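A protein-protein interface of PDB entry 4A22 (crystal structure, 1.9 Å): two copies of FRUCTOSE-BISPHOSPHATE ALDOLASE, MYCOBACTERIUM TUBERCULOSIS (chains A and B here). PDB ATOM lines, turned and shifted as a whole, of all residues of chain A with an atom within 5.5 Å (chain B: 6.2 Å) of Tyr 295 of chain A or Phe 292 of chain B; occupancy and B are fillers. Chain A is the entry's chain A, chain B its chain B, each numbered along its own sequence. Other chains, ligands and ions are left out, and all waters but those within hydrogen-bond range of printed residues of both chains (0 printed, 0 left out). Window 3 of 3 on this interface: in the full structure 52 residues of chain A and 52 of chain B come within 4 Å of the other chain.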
ATOM      1  N   HIS A 290      -2.451 -19.680  12.901  1.00  0.00           N
ATOM      2  CA  HIS A 290      -3.167 -18.444  13.196  1.00  0.00           C
ATOM      3  C   HIS A 290      -4.280 -18.695  14.224  1.00  0.00           C
ATOM      4  O   HIS A 290      -4.405 -17.952  15.202  1.00  0.00           O
ATOM      5  CB  HIS A 290      -3.774 -17.902  11.899  1.00  0.00           C
ATOM      6  CG  HIS A 290      -4.564 -16.632  12.062  1.00  0.00           C
ATOM      7  ND1 HIS A 290      -4.013 -15.384  11.878  1.00  0.00           N
ATOM      8  CD2 HIS A 290      -5.869 -16.416  12.379  1.00  0.00           C
ATOM      9  CE1 HIS A 290      -4.941 -14.451  12.040  1.00  0.00           C
ATOM     10  NE2 HIS A 290      -6.076 -15.057  12.346  1.00  0.00           N
ATOM     11  N   MET A 291      -5.086 -19.734  13.999  1.00  0.00           N
ATOM     12  CA  MET A 291      -6.225 -20.023  14.881  1.00  0.00           C
ATOM     13  C   MET A 291      -5.758 -20.319  16.316  1.00  0.00           C
ATOM     14  O   MET A 291      -6.392 -19.896  17.290  1.00  0.00           O
ATOM     15  CB  MET A 291      -7.040 -21.217  14.354  1.00  0.00           C
ATOM     16  CG  MET A 291      -7.665 -21.019  12.954  1.00  0.00           C
ATOM     17  SD  MET A 291      -8.637 -19.482  12.868  1.00  0.00           S
ATOM     18  CE  MET A 291      -8.862 -19.358  11.100  1.00  0.00           C
ATOM     19  N   PHE A 292      -4.667 -21.071  16.448  1.00  0.00           N
ATOM     20  CA  PHE A 292      -4.184 -21.465  17.788  1.00  0.00           C
ATOM     21  C   PHE A 292      -3.612 -20.257  18.520  1.00  0.00           C
ATOM     22  O   PHE A 292      -4.005 -19.955  19.622  1.00  0.00           O
ATOM     23  CB  PHE A 292      -3.142 -22.599  17.675  1.00  0.00           C
ATOM     24  CG  PHE A 292      -3.696 -23.854  17.032  1.00  0.00           C
ATOM     25  CD1 PHE A 292      -5.045 -24.161  17.133  1.00  0.00           C
ATOM     26  CD2 PHE A 292      -2.889 -24.697  16.299  1.00  0.00           C
ATOM     27  CE1 PHE A 292      -5.570 -25.308  16.542  1.00  0.00           C
ATOM     28  CE2 PHE A 292      -3.420 -25.852  15.697  1.00  0.00           C
ATOM     29  CZ  PHE A 292      -4.752 -26.154  15.833  1.00  0.00           C
ATOM     30  N   THR A 293      -2.715 -19.530  17.887  1.00  0.00           N
ATOM     31  CA  THR A 293      -2.091 -18.395  18.562  1.00  0.00           C
ATOM     32  C   THR A 293      -3.089 -17.264  18.858  1.00  0.00           C
ATOM     33  O   THR A 293      -2.925 -16.541  19.818  1.00  0.00           O
ATOM     34  CB  THR A 293      -0.900 -17.877  17.737  1.00  0.00           C
ATOM     35  OG1 THR A 293      -1.367 -17.333  16.503  1.00  0.00           O
ATOM     36  CG2 THR A 293       0.072 -19.035  17.430  1.00  0.00           C
ATOM     37  N   ASN A 294      -4.095 -17.123  18.001  1.00  0.00           N
ATOM     38  CA  ASN A 294      -5.163 -16.097  18.107  1.00  0.00           C
ATOM     39  C   ASN A 294      -6.468 -16.634  18.688  1.00  0.00           C
ATOM     40  O   ASN A 294      -7.540 -16.146  18.349  1.00  0.00           O
ATOM     41  CB  ASN A 294      -5.378 -15.381  16.783  1.00  0.00           C
ATOM     42  CG  ASN A 294      -4.136 -14.663  16.325  1.00  0.00           C
ATOM     43  OD1 ASN A 294      -3.657 -13.744  16.985  1.00  0.00           O
ATOM     44  ND2 ASN A 294      -3.584 -15.100  15.210  1.00  0.00           N
ATOM     45  N   TYR A 295      -6.386 -17.754  19.404  1.00  0.00           N
ATOM     46  CA  TYR A 295      -7.575 -18.473  19.830  1.00  0.00           C
ATOM     47  C   TYR A 295      -8.621 -17.560  20.481  1.00  0.00           C
ATOM     48  O   TYR A 295      -9.821 -17.778  20.327  1.00  0.00           O
ATOM     49  CB  TYR A 295      -7.192 -19.602  20.785  1.00  0.00           C
ATOM     50  CG  TYR A 295      -6.904 -19.136  22.180  1.00  0.00           C
ATOM     51  CD1 TYR A 295      -5.656 -18.669  22.528  1.00  0.00           C
ATOM     52  CD2 TYR A 295      -7.890 -19.181  23.163  1.00  0.00           C
ATOM     53  CE1 TYR A 295      -5.391 -18.235  23.813  1.00  0.00           C
ATOM     54  CE2 TYR A 295      -7.635 -18.757  24.452  1.00  0.00           C
ATOM     55  CZ  TYR A 295      -6.379 -18.292  24.771  1.00  0.00           C
ATOM     56  OH  TYR A 295      -6.111 -17.855  26.048  1.00  0.00           O
ATOM     57  N   ASP A 296      -8.160 -16.545  21.199  1.00  0.00           N
ATOM     58  CA  ASP A 296      -9.061 -15.718  21.975  1.00  0.00           C
ATOM     59  C   ASP A 296      -9.486 -14.469  21.201  1.00  0.00           C
ATOM     60  O   ASP A 296     -10.249 -13.672  21.709  1.00  0.00           O
ATOM     61  CB  ASP A 296      -8.472 -15.340  23.334  1.00  0.00           C
ATOM     62  CG  ASP A 296      -7.078 -14.795  23.239  1.00  0.00           C
ATOM     63  OD1 ASP A 296      -6.460 -14.902  22.159  1.00  0.00           O
ATOM     64  OD2 ASP A 296      -6.589 -14.276  24.268  1.00  0.00           O
ATOM     65  N   GLY A 297      -8.948 -14.274  20.001  1.00  0.00           N
ATOM     66  CA  GLY A 297      -9.506 -13.294  19.092  1.00  0.00           C
ATOM     67  C   GLY A 297     -10.366 -13.884  17.983  1.00  0.00           C
ATOM     68  O   GLY A 297     -11.308 -13.233  17.547  1.00  0.00           O
ATOM     69  N   VAL A 298     -10.107 -15.126  17.569  1.00  0.00           N
ATOM     70  CA  VAL A 298     -10.926 -15.749  16.535  1.00  0.00           C
ATOM     71  C   VAL A 298     -12.178 -16.361  17.131  1.00  0.00           C
ATOM     72  O   VAL A 298     -13.157 -16.563  16.421  1.00  0.00           O
ATOM     73  CB  VAL A 298     -10.167 -16.820  15.693  1.00  0.00           C
ATOM     74  CG1 VAL A 298      -8.890 -16.232  15.113  1.00  0.00           C
ATOM     75  CG2 VAL A 298      -9.858 -18.064  16.534  1.00  0.00           C
ATOM     76  N   LEU A 299     -12.146 -16.654  18.432  1.00  0.00           N
ATOM     77  CA  LEU A 299     -13.335 -17.111  19.139  1.00  0.00           C
ATOM     78  C   LEU A 299     -13.797 -15.996  20.072  1.00  0.00           C
ATOM     79  O   LEU A 299     -12.978 -15.236  20.593  1.00  0.00           O
ATOM     80  CB  LEU A 299     -13.032 -18.358  19.976  1.00  0.00           C
ATOM     81  CG  LEU A 299     -12.532 -19.614  19.250  1.00  0.00           C
ATOM     82  CD1 LEU A 299     -12.198 -20.723  20.255  1.00  0.00           C
ATOM     83  CD2 LEU A 299     -13.572 -20.097  18.254  1.00  0.00           C
ATOM     84  N   VAL A 301     -14.657 -15.335  23.552  1.00  0.00           N
ATOM     85  CA  VAL A 301     -14.404 -16.129  24.765  1.00  0.00           C
ATOM     86  C   VAL A 301     -14.623 -15.322  26.049  1.00  0.00           C
ATOM     87  O   VAL A 301     -14.350 -14.118  26.095  1.00  0.00           O
ATOM     88  CB  VAL A 301     -12.975 -16.734  24.760  1.00  0.00           C
ATOM     89  CG1 VAL A 301     -11.935 -15.652  24.626  1.00  0.00           C
ATOM     90  CG2 VAL A 301     -12.726 -17.544  26.025  1.00  0.00           C
ATOM     91  N   ILE B 287     -13.869 -22.620  10.780  1.00  0.00           N
ATOM     92  CA  ILE B 287     -12.484 -22.924  10.429  1.00  0.00           C
ATOM     93  C   ILE B 287     -11.697 -23.093  11.722  1.00  0.00           C
ATOM     94  O   ILE B 287     -10.976 -24.084  11.897  1.00  0.00           O
ATOM     95  CB  ILE B 287     -11.863 -21.836   9.529  1.00  0.00           C
ATOM     96  CG1 ILE B 287     -12.635 -21.764   8.202  1.00  0.00           C
ATOM     97  CG2 ILE B 287     -10.375 -22.135   9.260  1.00  0.00           C
ATOM     98  CD1 ILE B 287     -12.147 -20.677   7.261  1.00  0.00           C
ATOM     99  N   ALA B 288     -11.865 -22.155  12.644  1.00  0.00           N
ATOM    100  CA  ALA B 288     -11.238 -22.277  13.958  1.00  0.00           C
ATOM    101  C   ALA B 288     -11.605 -23.630  14.572  1.00  0.00           C
ATOM    102  O   ALA B 288     -10.728 -24.380  15.009  1.00  0.00           O
ATOM    103  CB  ALA B 288     -11.666 -21.135  14.872  1.00  0.00           C
ATOM    104  N   GLY B 289     -12.896 -23.942  14.605  1.00  0.00           N
ATOM    105  CA  GLY B 289     -13.364 -25.204  15.170  1.00  0.00           C
ATOM    106  C   GLY B 289     -12.705 -26.413  14.525  1.00  0.00           C
ATOM    107  O   GLY B 289     -12.228 -27.339  15.214  1.00  0.00           O
ATOM    108  N   HIS B 290     -12.660 -26.402  13.195  1.00  0.00           N
ATOM    109  CA  HIS B 290     -11.992 -27.454  12.428  1.00  0.00           C
ATOM    110  C   HIS B 290     -10.546 -27.658  12.859  1.00  0.00           C
ATOM    111  O   HIS B 290     -10.099 -28.793  13.054  1.00  0.00           O
ATOM    112  CB  HIS B 290     -12.003 -27.078  10.954  1.00  0.00           C
ATOM    113  CG  HIS B 290     -11.415 -28.121  10.045  1.00  0.00           C
ATOM    114  ND1 HIS B 290     -12.166 -29.137   9.511  1.00  0.00           N
ATOM    115  CD2 HIS B 290     -10.167 -28.262   9.535  1.00  0.00           C
ATOM    116  CE1 HIS B 290     -11.407 -29.873   8.708  1.00  0.00           C
ATOM    117  NE2 HIS B 290     -10.193 -29.363   8.708  1.00  0.00           N
ATOM    118  N   MET B 291      -9.800 -26.562  12.986  1.00  0.00           N
ATOM    119  CA  MET B 291      -8.380 -26.664  13.324  1.00  0.00           C
ATOM    120  C   MET B 291      -8.179 -27.242  14.727  1.00  0.00           C
ATOM    121  O   MET B 291      -7.308 -28.080  14.925  1.00  0.00           O
ATOM    122  CB  MET B 291      -7.705 -25.300  13.204  1.00  0.00           C
ATOM    123  CG  MET B 291      -7.818 -24.702  11.783  1.00  0.00           C
ATOM    124  SD  MET B 291      -7.094 -25.759  10.499  1.00  0.00           S
ATOM    125  CE  MET B 291      -7.761 -24.922   9.040  1.00  0.00           C
ATOM    126  N   PHE B 292      -9.002 -26.812  15.685  1.00  0.00           N
ATOM    127  CA  PHE B 292      -8.893 -27.322  17.059  1.00  0.00           C
ATOM    128  C   PHE B 292      -9.234 -28.812  17.104  1.00  0.00           C
ATOM    129  O   PHE B 292      -8.433 -29.618  17.593  1.00  0.00           O
ATOM    130  CB  PHE B 292      -9.792 -26.530  18.030  1.00  0.00           C
ATOM    131  CG  PHE B 292      -9.303 -25.133  18.313  1.00  0.00           C
ATOM    132  CD1 PHE B 292      -8.198 -24.919  19.124  1.00  0.00           C
ATOM    133  CD2 PHE B 292      -9.961 -24.031  17.793  1.00  0.00           C
ATOM    134  CE1 PHE B 292      -7.748 -23.629  19.383  1.00  0.00           C
ATOM    135  CE2 PHE B 292      -9.502 -22.746  18.035  1.00  0.00           C
ATOM    136  CZ  PHE B 292      -8.402 -22.543  18.818  1.00  0.00           C
ATOM    137  N   THR B 293     -10.409 -29.192  16.593  1.00  0.00           N
ATOM    138  CA  THR B 293     -10.850 -30.577  16.743  1.00  0.00           C
ATOM    139  C   THR B 293      -9.958 -31.526  15.944  1.00  0.00           C
ATOM    140  O   THR B 293      -9.752 -32.660  16.339  1.00  0.00           O
ATOM    141  CB  THR B 293     -12.337 -30.785  16.357  1.00  0.00           C
ATOM    142  OG1 THR B 293     -12.509 -30.583  14.958  1.00  0.00           O
ATOM    143  CG2 THR B 293     -13.241 -29.829  17.121  1.00  0.00           C
ATOM    144  N   ASN B 294      -9.438 -31.042  14.821  1.00  0.00           N
ATOM    145  CA  ASN B 294      -8.510 -31.778  13.961  1.00  0.00           C
ATOM    146  C   ASN B 294      -7.002 -31.486  14.156  1.00  0.00           C
ATOM    147  O   ASN B 294      -6.220 -31.643  13.225  1.00  0.00           O
ATOM    148  CB  ASN B 294      -8.936 -31.663  12.495  1.00  0.00           C
ATOM    149  CG  ASN B 294     -10.302 -32.239  12.264  1.00  0.00           C
ATOM    150  OD1 ASN B 294     -10.499 -33.429  12.426  1.00  0.00           O
ATOM    151  ND2 ASN B 294     -11.270 -31.392  11.931  1.00  0.00           N
ATOM    152  N   TYR B 295      -6.616 -30.930  15.299  1.00  0.00           N
ATOM    153  CA  TYR B 295      -5.263 -30.401  15.478  1.00  0.00           C
ATOM    154  C   TYR B 295      -4.165 -31.378  15.029  1.00  0.00           C
ATOM    155  O   TYR B 295      -3.147 -30.976  14.488  1.00  0.00           O
ATOM    156  CB  TYR B 295      -5.048 -29.993  16.941  1.00  0.00           C
ATOM    157  CG  TYR B 295      -4.745 -31.169  17.833  1.00  0.00           C
ATOM    158  CD1 TYR B 295      -5.763 -32.026  18.237  1.00  0.00           C
ATOM    159  CD2 TYR B 295      -3.430 -31.465  18.222  1.00  0.00           C
ATOM    160  CE1 TYR B 295      -5.500 -33.124  19.046  1.00  0.00           C
ATOM    161  CE2 TYR B 295      -3.157 -32.569  19.038  1.00  0.00           C
ATOM    162  CZ  TYR B 295      -4.196 -33.401  19.424  1.00  0.00           C
ATOM    163  OH  TYR B 295      -3.978 -34.501  20.222  1.00  0.00           O
ATOM    164  N   ASP B 296      -4.383 -32.667  15.229  1.00  0.00           N
ATOM    165  CA  ASP B 296      -3.342 -33.642  14.945  1.00  0.00           C
ATOM    166  C   ASP B 296      -3.481 -34.213  13.529  1.00  0.00           C
ATOM    167  O   ASP B 296      -2.717 -35.091  13.148  1.00  0.00           O
ATOM    168  CB  ASP B 296      -3.357 -34.758  15.997  1.00  0.00           C
ATOM    169  CG  ASP B 296      -4.661 -35.532  16.014  1.00  0.00           C
ATOM    170  OD1 ASP B 296      -5.689 -35.012  15.514  1.00  0.00           O
ATOM    171  OD2 ASP B 296      -4.657 -36.675  16.519  1.00  0.00           O
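Printed residues of chain B that touch a printed residue of chain A: Ile 287, Ala 288, Met 291 and Phe 292.
Hydrophobic or aromatic side chains of chain B within 4 Å of the printed part of chain A: Ile 287, Ala 288, Met 291 and Phe 292.
Printed residues of chain B within 4 Å of Phe 292 of chain A: Met 291 and Phe 292.
Of chain B, only Phe 292 (3.7 Å) comes within 4 Å of Tyr 295 of chain A.
Printed residues of chain B within 4 Å of Val 298 of chain A: Ala 288 (3.9 Å).
Printed residues of chain A within 4 Å of Ile 287 of chain B: Met 291 (3.7 Å).
Of the printed residues of chain A, Ala 288 of chain B touches Met 291 (3.9 Å) and Val 298 (3.9 Å).
Of the printed residues of chain A, Met 291 of chain B touches Met 291 (3.9 Å) and Phe 292 (3.3 Å).
Thr 293 of chain B touches none of the printed residues of chain A.
Asn 294 of chain B touches none of the printed residues of chain A.
Ile 287 of chain B touches Met 291 of chain A.
Met 291 of chain A touches Ala 288 of chain B.
CG of Met 291 of chain A touches CG of Met 291 of chain B, at 3.9 Å.
Met 291 of chain A touches Phe 292 of chain B.
O of Met 291 of chain B touches CZ of Phe 292 of chain A (3.3 Å).
Phe 292 of chain A touches Phe 292 of chain B (CD1 to CE1, 3.6 Å).
CZ of Phe 292 of chain B touches CB of Tyr 295 of chain A (3.7 Å).
Val 298 of chain A touches Ala 288 of chain B.
Met 291 of chain A touches its own counterpart, Met 291 of chain B.
Met 291 of chain A touches Phe 292 of chain B, and with the chains exchanged Phe 292 of chain A touches Met 291 of chain B.
Phe 292 of chain B touches its own counterpart, Phe 292 of chain A.
Tyr 295 of chain A touches Phe 292 of chain B, but with the chains exchanged Phe 292 of chain A does not touch Tyr 295 of chain B (4.01 Å).
7 positions are printed for both chains.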
